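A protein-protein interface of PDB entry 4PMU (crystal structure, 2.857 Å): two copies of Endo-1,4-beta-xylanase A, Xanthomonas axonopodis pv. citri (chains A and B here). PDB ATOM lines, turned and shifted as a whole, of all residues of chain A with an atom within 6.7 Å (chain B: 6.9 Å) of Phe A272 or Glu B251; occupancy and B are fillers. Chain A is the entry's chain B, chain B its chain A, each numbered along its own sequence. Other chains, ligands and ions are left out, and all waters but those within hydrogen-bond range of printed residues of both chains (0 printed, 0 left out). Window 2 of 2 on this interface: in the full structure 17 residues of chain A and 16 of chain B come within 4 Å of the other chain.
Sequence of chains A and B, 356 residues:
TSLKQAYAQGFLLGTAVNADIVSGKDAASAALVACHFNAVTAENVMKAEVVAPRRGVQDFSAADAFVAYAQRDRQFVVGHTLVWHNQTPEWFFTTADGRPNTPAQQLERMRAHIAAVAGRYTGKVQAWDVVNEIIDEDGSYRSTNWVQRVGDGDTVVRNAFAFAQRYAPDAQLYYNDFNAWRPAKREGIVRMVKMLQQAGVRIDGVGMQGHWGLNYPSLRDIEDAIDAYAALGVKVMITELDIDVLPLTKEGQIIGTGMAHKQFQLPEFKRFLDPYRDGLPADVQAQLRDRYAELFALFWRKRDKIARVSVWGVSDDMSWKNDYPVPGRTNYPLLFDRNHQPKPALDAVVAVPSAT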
ATOM      1  N   LEU A 246     -16.034  41.036  25.972  1.00  0.00           N
ATOM      2  CA  LEU A 246     -16.226  39.593  26.132  1.00  0.00           C
ATOM      3  C   LEU A 246     -17.065  39.010  25.003  1.00  0.00           C
ATOM      4  O   LEU A 246     -17.847  39.735  24.384  1.00  0.00           O
ATOM      5  CB  LEU A 246     -16.875  39.282  27.479  1.00  0.00           C
ATOM      6  CG  LEU A 246     -16.120  39.695  28.738  1.00  0.00           C
ATOM      7  CD1 LEU A 246     -16.903  39.255  29.962  1.00  0.00           C
ATOM      8  CD2 LEU A 246     -14.721  39.104  28.744  1.00  0.00           C
ATOM      9  N   PRO A 247     -16.907  37.697  24.731  1.00  0.00           N
ATOM     10  CA  PRO A 247     -17.625  37.035  23.635  1.00  0.00           C
ATOM     11  C   PRO A 247     -19.143  37.193  23.698  1.00  0.00           C
ATOM     12  O   PRO A 247     -19.704  37.391  24.779  1.00  0.00           O
ATOM     13  CB  PRO A 247     -17.217  35.570  23.795  1.00  0.00           C
ATOM     14  CG  PRO A 247     -15.839  35.650  24.362  1.00  0.00           C
ATOM     15  CD  PRO A 247     -15.902  36.796  25.334  1.00  0.00           C
ATOM     16  N   LEU A 248     -19.777  37.111  22.527  1.00  0.00           N
ATOM     17  CA  LEU A 248     -21.225  37.338  22.333  1.00  0.00           C
ATOM     18  C   LEU A 248     -21.668  38.790  22.551  1.00  0.00           C
ATOM     19  O   LEU A 248     -22.331  39.378  21.695  1.00  0.00           O
ATOM     20  CB  LEU A 248     -22.084  36.376  23.177  1.00  0.00           C
ATOM     21  CG  LEU A 248     -23.596  36.392  22.911  1.00  0.00           C
ATOM     22  CD1 LEU A 248     -23.942  35.825  21.538  1.00  0.00           C
ATOM     23  CD2 LEU A 248     -24.340  35.640  24.001  1.00  0.00           C
ATOM     24  N   PRO A 267     -19.891  24.691  32.895  1.00  0.00           N
ATOM     25  CA  PRO A 267     -18.474  24.763  32.525  1.00  0.00           C
ATOM     26  C   PRO A 267     -18.167  24.966  31.039  1.00  0.00           C
ATOM     27  O   PRO A 267     -17.178  25.619  30.721  1.00  0.00           O
ATOM     28  CB  PRO A 267     -17.925  23.423  33.007  1.00  0.00           C
ATOM     29  CG  PRO A 267     -18.767  23.111  34.194  1.00  0.00           C
ATOM     30  CD  PRO A 267     -20.146  23.562  33.810  1.00  0.00           C
ATOM     31  N   GLU A 268     -18.988  24.426  30.142  1.00  0.00           N
ATOM     32  CA  GLU A 268     -18.719  24.588  28.708  1.00  0.00           C
ATOM     33  C   GLU A 268     -18.997  26.008  28.220  1.00  0.00           C
ATOM     34  O   GLU A 268     -18.359  26.479  27.277  1.00  0.00           O
ATOM     35  CB  GLU A 268     -19.467  23.557  27.851  1.00  0.00           C
ATOM     36  CG  GLU A 268     -20.984  23.601  27.958  1.00  0.00           C
ATOM     37  CD  GLU A 268     -21.528  22.672  29.026  1.00  0.00           C
ATOM     38  OE1 GLU A 268     -20.735  22.196  29.877  1.00  0.00           O
ATOM     39  OE2 GLU A 268     -22.756  22.412  29.012  1.00  0.00           O
ATOM     40  N   PHE A 269     -19.945  26.682  28.869  1.00  0.00           N
ATOM     41  CA  PHE A 269     -20.303  28.048  28.496  1.00  0.00           C
ATOM     42  C   PHE A 269     -19.435  29.081  29.197  1.00  0.00           C
ATOM     43  O   PHE A 269     -18.979  30.032  28.564  1.00  0.00           O
ATOM     44  CB  PHE A 269     -21.794  28.325  28.734  1.00  0.00           C
ATOM     45  CG  PHE A 269     -22.692  27.723  27.690  1.00  0.00           C
ATOM     46  CD1 PHE A 269     -22.625  28.146  26.365  1.00  0.00           C
ATOM     47  CD2 PHE A 269     -23.600  26.730  28.024  1.00  0.00           C
ATOM     48  CE1 PHE A 269     -23.443  27.587  25.399  1.00  0.00           C
ATOM     49  CE2 PHE A 269     -24.424  26.170  27.065  1.00  0.00           C
ATOM     50  CZ  PHE A 269     -24.346  26.601  25.752  1.00  0.00           C
ATOM     51  N   LYS A 270     -19.198  28.887  30.493  1.00  0.00           N
ATOM     52  CA  LYS A 270     -18.300  29.763  31.248  1.00  0.00           C
ATOM     53  C   LYS A 270     -16.927  29.797  30.572  1.00  0.00           C
ATOM     54  O   LYS A 270     -16.307  30.854  30.459  1.00  0.00           O
ATOM     55  CB  LYS A 270     -18.196  29.320  32.715  1.00  0.00           C
ATOM     56  CG  LYS A 270     -17.580  30.372  33.629  1.00  0.00           C
ATOM     57  CD  LYS A 270     -18.002  30.187  35.080  1.00  0.00           C
ATOM     58  CE  LYS A 270     -17.140  31.017  36.033  1.00  0.00           C
ATOM     59  NZ  LYS A 270     -17.308  32.496  35.908  1.00  0.00           N
ATOM     60  N   ARG A 271     -16.487  28.628  30.110  1.00  0.00           N
ATOM     61  CA  ARG A 271     -15.271  28.460  29.315  1.00  0.00           C
ATOM     62  C   ARG A 271     -15.221  29.437  28.137  1.00  0.00           C
ATOM     63  O   ARG A 271     -14.200  30.083  27.900  1.00  0.00           O
ATOM     64  CB  ARG A 271     -15.220  27.019  28.797  1.00  0.00           C
ATOM     65  CG  ARG A 271     -13.875  26.535  28.287  1.00  0.00           C
ATOM     66  CD  ARG A 271     -14.023  25.165  27.642  1.00  0.00           C
ATOM     67  NE  ARG A 271     -12.770  24.709  27.042  1.00  0.00           N
ATOM     68  CZ  ARG A 271     -12.680  23.799  26.075  1.00  0.00           C
ATOM     69  NH1 ARG A 271     -13.776  23.236  25.574  1.00  0.00           N
ATOM     70  NH2 ARG A 271     -11.486  23.455  25.600  1.00  0.00           N
ATOM     71  N   PHE A 272     -16.336  29.543  27.417  1.00  0.00           N
ATOM     72  CA  PHE A 272     -16.436  30.361  26.209  1.00  0.00           C
ATOM     73  C   PHE A 272     -16.721  31.840  26.491  1.00  0.00           C
ATOM     74  O   PHE A 272     -16.106  32.722  25.887  1.00  0.00           O
ATOM     75  CB  PHE A 272     -17.522  29.784  25.298  1.00  0.00           C
ATOM     76  CG  PHE A 272     -17.863  30.654  24.119  1.00  0.00           C
ATOM     77  CD1 PHE A 272     -16.945  30.850  23.085  1.00  0.00           C
ATOM     78  CD2 PHE A 272     -19.111  31.264  24.031  1.00  0.00           C
ATOM     79  CE1 PHE A 272     -17.263  31.647  21.996  1.00  0.00           C
ATOM     80  CE2 PHE A 272     -19.433  32.061  22.942  1.00  0.00           C
ATOM     81  CZ  PHE A 272     -18.510  32.253  21.925  1.00  0.00           C
ATOM     82  N   LEU A 273     -17.656  32.095  27.406  1.00  0.00           N
ATOM     83  CA  LEU A 273     -18.155  33.437  27.683  1.00  0.00           C
ATOM     84  C   LEU A 273     -17.251  34.244  28.611  1.00  0.00           C
ATOM     85  O   LEU A 273     -17.297  35.477  28.611  1.00  0.00           O
ATOM     86  CB  LEU A 273     -19.558  33.364  28.293  1.00  0.00           C
ATOM     87  CG  LEU A 273     -20.696  32.687  27.528  1.00  0.00           C
ATOM     88  CD1 LEU A 273     -21.865  32.423  28.465  1.00  0.00           C
ATOM     89  CD2 LEU A 273     -21.136  33.518  26.331  1.00  0.00           C
ATOM     90  N   ASP A 274     -16.442  33.550  29.405  1.00  0.00           N
ATOM     91  CA  ASP A 274     -15.605  34.203  30.402  1.00  0.00           C
ATOM     92  C   ASP A 274     -14.140  33.765  30.272  1.00  0.00           C
ATOM     93  O   ASP A 274     -13.603  33.098  31.166  1.00  0.00           O
ATOM     94  CB  ASP A 274     -16.148  33.914  31.805  1.00  0.00           C
ATOM     95  CG  ASP A 274     -15.730  34.959  32.825  1.00  0.00           C
ATOM     96  OD1 ASP A 274     -15.252  36.045  32.416  1.00  0.00           O
ATOM     97  OD2 ASP A 274     -15.886  34.696  34.041  1.00  0.00           O
ATOM     98  N   PRO A 275     -13.481  34.148  29.160  1.00  0.00           N
ATOM     99  CA  PRO A 275     -12.153  33.621  28.876  1.00  0.00           C
ATOM    100  C   PRO A 275     -11.007  34.425  29.496  1.00  0.00           C
ATOM    101  O   PRO A 275      -9.870  33.946  29.522  1.00  0.00           O
ATOM    102  CB  PRO A 275     -12.080  33.678  27.348  1.00  0.00           C
ATOM    103  CG  PRO A 275     -13.066  34.733  26.937  1.00  0.00           C
ATOM    104  CD  PRO A 275     -13.909  35.107  28.126  1.00  0.00           C
ATOM    105  N   ARG A 277     -10.286  35.693  32.749  1.00  0.00           N
ATOM    106  CA  ARG A 277     -10.437  35.754  34.203  1.00  0.00           C
ATOM    107  C   ARG A 277      -9.138  36.117  34.939  1.00  0.00           C
ATOM    108  O   ARG A 277      -9.122  36.209  36.171  1.00  0.00           O
ATOM    109  CB  ARG A 277     -11.026  34.438  34.738  1.00  0.00           C
ATOM    110  CG  ARG A 277     -12.550  34.406  34.809  1.00  0.00           C
ATOM    111  CD  ARG A 277     -13.076  33.040  35.236  1.00  0.00           C
ATOM    112  NE  ARG A 277     -13.125  32.106  34.106  1.00  0.00           N
ATOM    113  CZ  ARG A 277     -13.457  30.816  34.184  1.00  0.00           C
ATOM    114  NH1 ARG A 277     -13.773  30.262  35.349  1.00  0.00           N
ATOM    115  NH2 ARG A 277     -13.467  30.074  33.086  1.00  0.00           N
ATOM    116  N   ARG A 329     -19.092  37.082  35.510  1.00  0.00           N
ATOM    117  CA  ARG A 329     -18.049  37.264  34.505  1.00  0.00           C
ATOM    118  C   ARG A 329     -17.082  38.377  34.872  1.00  0.00           C
ATOM    119  O   ARG A 329     -17.372  39.223  35.720  1.00  0.00           O
ATOM    120  CB  ARG A 329     -18.654  37.540  33.132  1.00  0.00           C
ATOM    121  CG  ARG A 329     -19.094  36.299  32.382  1.00  0.00           C
ATOM    122  CD  ARG A 329     -20.167  36.689  31.391  1.00  0.00           C
ATOM    123  NE  ARG A 329     -19.703  36.792  30.013  1.00  0.00           N
ATOM    124  CZ  ARG A 329     -20.169  37.671  29.132  1.00  0.00           C
ATOM    125  NH1 ARG A 329     -21.084  38.562  29.493  1.00  0.00           N
ATOM    126  NH2 ARG A 329     -19.700  37.673  27.891  1.00  0.00           N
ATOM    127  N   GLY B 213     -21.310  19.608  19.398  1.00  0.00           N
ATOM    128  CA  GLY B 213     -20.747  20.611  18.499  1.00  0.00           C
ATOM    129  C   GLY B 213     -19.268  20.411  18.235  1.00  0.00           C
ATOM    130  O   GLY B 213     -18.712  19.352  18.531  1.00  0.00           O
ATOM    131  N   LEU B 214     -18.633  21.436  17.678  1.00  0.00           N
ATOM    132  CA  LEU B 214     -17.210  21.380  17.346  1.00  0.00           C
ATOM    133  C   LEU B 214     -16.316  21.465  18.587  1.00  0.00           C
ATOM    134  O   LEU B 214     -15.270  20.817  18.648  1.00  0.00           O
ATOM    135  CB  LEU B 214     -16.843  22.478  16.336  1.00  0.00           C
ATOM    136  CG  LEU B 214     -17.460  22.399  14.931  1.00  0.00           C
ATOM    137  CD1 LEU B 214     -17.427  23.752  14.244  1.00  0.00           C
ATOM    138  CD2 LEU B 214     -16.778  21.345  14.068  1.00  0.00           C
ATOM    139  N   ASN B 215     -16.739  22.248  19.577  1.00  0.00           N
ATOM    140  CA  ASN B 215     -15.931  22.474  20.777  1.00  0.00           C
ATOM    141  C   ASN B 215     -16.472  21.833  22.058  1.00  0.00           C
ATOM    142  O   ASN B 215     -16.046  22.182  23.161  1.00  0.00           O
ATOM    143  CB  ASN B 215     -15.699  23.976  20.985  1.00  0.00           C
ATOM    144  CG  ASN B 215     -14.889  24.609  19.865  1.00  0.00           C
ATOM    145  OD1 ASN B 215     -14.222  23.918  19.088  1.00  0.00           O
ATOM    146  ND2 ASN B 215     -14.943  25.932  19.778  1.00  0.00           N
ATOM    147  N   TYR B 216     -17.402  20.894  21.910  1.00  0.00           N
ATOM    148  CA  TYR B 216     -17.965  20.183  23.056  1.00  0.00           C
ATOM    149  C   TYR B 216     -18.628  18.874  22.611  1.00  0.00           C
ATOM    150  O   TYR B 216     -19.138  18.789  21.489  1.00  0.00           O
ATOM    151  CB  TYR B 216     -18.957  21.080  23.820  1.00  0.00           C
ATOM    152  CG  TYR B 216     -20.396  20.964  23.373  1.00  0.00           C
ATOM    153  CD1 TYR B 216     -20.832  21.567  22.198  1.00  0.00           C
ATOM    154  CD2 TYR B 216     -21.317  20.248  24.128  1.00  0.00           C
ATOM    155  CE1 TYR B 216     -22.150  21.457  21.786  1.00  0.00           C
ATOM    156  CE2 TYR B 216     -22.636  20.131  23.726  1.00  0.00           C
ATOM    157  CZ  TYR B 216     -23.046  20.735  22.555  1.00  0.00           C
ATOM    158  OH  TYR B 216     -24.352  20.615  22.147  1.00  0.00           O
ATOM    159  N   PRO B 217     -18.591  17.837  23.471  1.00  0.00           N
ATOM    160  CA  PRO B 217     -17.857  17.752  24.733  1.00  0.00           C
ATOM    161  C   PRO B 217     -16.493  17.089  24.554  1.00  0.00           C
ATOM    162  O   PRO B 217     -16.126  16.732  23.438  1.00  0.00           O
ATOM    163  CB  PRO B 217     -18.755  16.862  25.586  1.00  0.00           C
ATOM    164  CG  PRO B 217     -19.478  15.988  24.611  1.00  0.00           C
ATOM    165  CD  PRO B 217     -19.419  16.637  23.252  1.00  0.00           C
ATOM    166  N   ASP B 244     -23.300  20.691  15.757  1.00  0.00           N
ATOM    167  CA  ASP B 244     -23.581  22.113  15.576  1.00  0.00           C
ATOM    168  C   ASP B 244     -22.293  22.873  15.288  1.00  0.00           C
ATOM    169  O   ASP B 244     -21.321  22.761  16.033  1.00  0.00           O
ATOM    170  CB  ASP B 244     -24.258  22.667  16.831  1.00  0.00           C
ATOM    171  CG  ASP B 244     -24.950  23.994  16.593  1.00  0.00           C
ATOM    172  OD1 ASP B 244     -24.326  24.915  16.010  1.00  0.00           O
ATOM    173  OD2 ASP B 244     -26.119  24.126  17.014  1.00  0.00           O
ATOM    174  N   LEU B 246     -22.244  26.381  14.335  1.00  0.00           N
ATOM    175  CA  LEU B 246     -22.467  27.829  14.354  1.00  0.00           C
ATOM    176  C   LEU B 246     -22.008  28.482  15.668  1.00  0.00           C
ATOM    177  O   LEU B 246     -21.909  27.796  16.689  1.00  0.00           O
ATOM    178  CB  LEU B 246     -23.941  28.132  14.065  1.00  0.00           C
ATOM    179  CG  LEU B 246     -24.490  27.754  12.686  1.00  0.00           C
ATOM    180  CD1 LEU B 246     -25.941  28.184  12.572  1.00  0.00           C
ATOM    181  CD2 LEU B 246     -23.671  28.374  11.565  1.00  0.00           C
ATOM    182  N   PRO B 247     -21.721  29.804  15.647  1.00  0.00           N
ATOM    183  CA  PRO B 247     -21.226  30.516  16.834  1.00  0.00           C
ATOM    184  C   PRO B 247     -22.132  30.345  18.047  1.00  0.00           C
ATOM    185  O   PRO B 247     -23.347  30.209  17.900  1.00  0.00           O
ATOM    186  CB  PRO B 247     -21.222  31.978  16.390  1.00  0.00           C
ATOM    187  CG  PRO B 247     -21.037  31.908  14.918  1.00  0.00           C
ATOM    188  CD  PRO B 247     -21.825  30.708  14.487  1.00  0.00           C
ATOM    189  N   LEU B 248     -21.529  30.349  19.233  1.00  0.00           N
ATOM    190  CA  LEU B 248     -22.232  30.099  20.499  1.00  0.00           C
ATOM    191  C   LEU B 248     -22.697  28.653  20.668  1.00  0.00           C
ATOM    192  O   LEU B 248     -22.361  28.012  21.662  1.00  0.00           O
ATOM    193  CB  LEU B 248     -23.404  31.071  20.716  1.00  0.00           C
ATOM    194  CG  LEU B 248     -24.281  30.835  21.951  1.00  0.00           C
ATOM    195  CD1 LEU B 248     -23.512  31.066  23.242  1.00  0.00           C
ATOM    196  CD2 LEU B 248     -25.506  31.728  21.900  1.00  0.00           C
ATOM    197  N   THR B 249     -23.469  28.153  19.708  1.00  0.00           N
ATOM    198  CA  THR B 249     -24.081  26.828  19.827  1.00  0.00           C
ATOM    199  C   THR B 249     -23.089  25.680  19.649  1.00  0.00           C
ATOM    200  O   THR B 249     -23.344  24.562  20.097  1.00  0.00           O
ATOM    201  CB  THR B 249     -25.256  26.650  18.854  1.00  0.00           C
ATOM    202  OG1 THR B 249     -24.830  26.997  17.531  1.00  0.00           O
ATOM    203  CG2 THR B 249     -26.428  27.534  19.260  1.00  0.00           C
ATOM    204  N   LYS B 250     -21.954  25.963  19.011  1.00  0.00           N
ATOM    205  CA  LYS B 250     -20.883  24.975  18.881  1.00  0.00           C
ATOM    206  C   LYS B 250     -20.123  24.796  20.200  1.00  0.00           C
ATOM    207  O   LYS B 250     -19.331  23.863  20.350  1.00  0.00           O
ATOM    208  CB  LYS B 250     -19.920  25.362  17.752  1.00  0.00           C
ATOM    209  CG  LYS B 250     -19.032  26.556  18.058  1.00  0.00           C
ATOM    210  CD  LYS B 250     -18.390  27.102  16.794  1.00  0.00           C
ATOM    211  CE  LYS B 250     -17.369  28.181  17.123  1.00  0.00           C
ATOM    212  NZ  LYS B 250     -16.979  28.924  15.896  1.00  0.00           N
ATOM    213  N   GLU B 251     -20.377  25.694  21.149  1.00  0.00           N
ATOM    214  CA  GLU B 251     -19.661  25.712  22.419  1.00  0.00           C
ATOM    215  C   GLU B 251     -20.362  24.905  23.510  1.00  0.00           C
ATOM    216  O   GLU B 251     -19.715  24.410  24.431  1.00  0.00           O
ATOM    217  CB  GLU B 251     -19.436  27.154  22.889  1.00  0.00           C
ATOM    218  CG  GLU B 251     -18.931  28.116  21.815  1.00  0.00           C
ATOM    219  CD  GLU B 251     -17.515  27.822  21.332  1.00  0.00           C
ATOM    220  OE1 GLU B 251     -16.861  26.910  21.889  1.00  0.00           O
ATOM    221  OE2 GLU B 251     -17.055  28.509  20.388  1.00  0.00           O
ATOM    222  N   GLY B 252     -21.680  24.780  23.404  1.00  0.00           N
ATOM    223  CA  GLY B 252     -22.477  24.006  24.358  1.00  0.00           C
ATOM    224  C   GLY B 252     -23.920  23.877  23.898  1.00  0.00           C
ATOM    225  O   GLY B 252     -24.371  24.640  23.038  1.00  0.00           O
ATOM    226  N   GLN B 253     -24.644  22.912  24.462  1.00  0.00           N
ATOM    227  CA  GLN B 253     -26.049  22.699  24.106  1.00  0.00           C
ATOM    228  C   GLN B 253     -26.928  23.691  24.860  1.00  0.00           C
ATOM    229  O   GLN B 253     -26.757  23.883  26.064  1.00  0.00           O
ATOM    230  CB  GLN B 253     -26.484  21.257  24.400  1.00  0.00           C
ATOM    231  CG  GLN B 253     -27.703  20.799  23.607  1.00  0.00           C
ATOM    232  CD  GLN B 253     -28.144  19.379  23.934  1.00  0.00           C
ATOM    233  OE1 GLN B 253     -27.324  18.495  24.188  1.00  0.00           O
ATOM    234  NE2 GLN B 253     -29.451  19.153  23.914  1.00  0.00           N
ATOM    235  N   PHE B 272     -23.693  37.750  13.104  1.00  0.00           N
ATOM    236  CA  PHE B 272     -22.719  37.023  13.910  1.00  0.00           C
ATOM    237  C   PHE B 272     -23.137  35.572  14.133  1.00  0.00           C
ATOM    238  O   PHE B 272     -22.333  34.660  13.936  1.00  0.00           O
ATOM    239  CB  PHE B 272     -22.487  37.729  15.250  1.00  0.00           C
ATOM    240  CG  PHE B 272     -21.826  36.864  16.290  1.00  0.00           C
ATOM    241  CD1 PHE B 272     -20.464  36.576  16.217  1.00  0.00           C
ATOM    242  CD2 PHE B 272     -22.564  36.340  17.345  1.00  0.00           C
ATOM    243  CE1 PHE B 272     -19.852  35.779  17.175  1.00  0.00           C
ATOM    244  CE2 PHE B 272     -21.959  35.540  18.303  1.00  0.00           C
ATOM    245  CZ  PHE B 272     -20.601  35.259  18.218  1.00  0.00           C
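Of the 15 printed residues of chain B, 6 touch a printed residue of chain A. Hydrophobic or aromatic side chains of chain B within 4 Å of the printed part of chain A: Phe B272. Hydrophobic or aromatic side chains of chain A that line the printed part of chain B: Leu A248, Phe A269 and Phe A272. Along chain A the printed residues that touch a printed residue of chain B span positions 248 to 272.
Of the printed residues of chain B, Leu A248 touches Phe B272 (3.8 Å). Of the printed residues of chain B, Glu A268 touches Glu B251 (3.5 Å) and Gly B252 (3.9 Å). Lys A270 touches none of the printed residues of chain B. Phe A272 touches just one residue of chain B: Glu B251 (3.5 Å). Leu B214 touches none of the printed residues of chain A. The nearest residue of chain B that does not touch Phe A272 is Leu B248 (4.2 Å). The nearest printed residue of chain A that does not touch Gln B253 is Glu A268 (5.0 Å).
The backbone carbonyl oxygen of Lys B250 lies within hydrogen-bond range of the backbone NH of Asn B215, 3.2 Å away. ND2 of Asn B215 lies within hydrogen-bond range of OE1 of Glu B251 (3.0 Å). OH of Tyr B216 sits close to N of Gln B253 (3.3 Å).
Leu A248 touches Phe B272. Glu B251 touches Glu A268 (O to CB, 3.5 Å). Glu A268 touches Gly B252. Leu B248 touches Phe A269 (O to CE1, 3.9 Å). Phe A269 touches Gly B252 (CZ to C, 3.3 Å). CE2 of Phe A269 touches O of Gln B253 (3.4 Å). Phe A272 touches Glu B251 (CE1 to OE2, 3.5 Å).
O of Asn B215 sits at hydrogen-bond distance from NH1 of Arg A271 (3.5 Å).
Leu A248 touches Phe B272, but with the chains exchanged Phe A272 does not touch Leu B248 (4.2 Å). Positions printed for both chains: 246, 247, 248 and 272. Of the 8 pairs that touch across the chains among the printed residues, none has its exchanged pair printed and touching as well.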
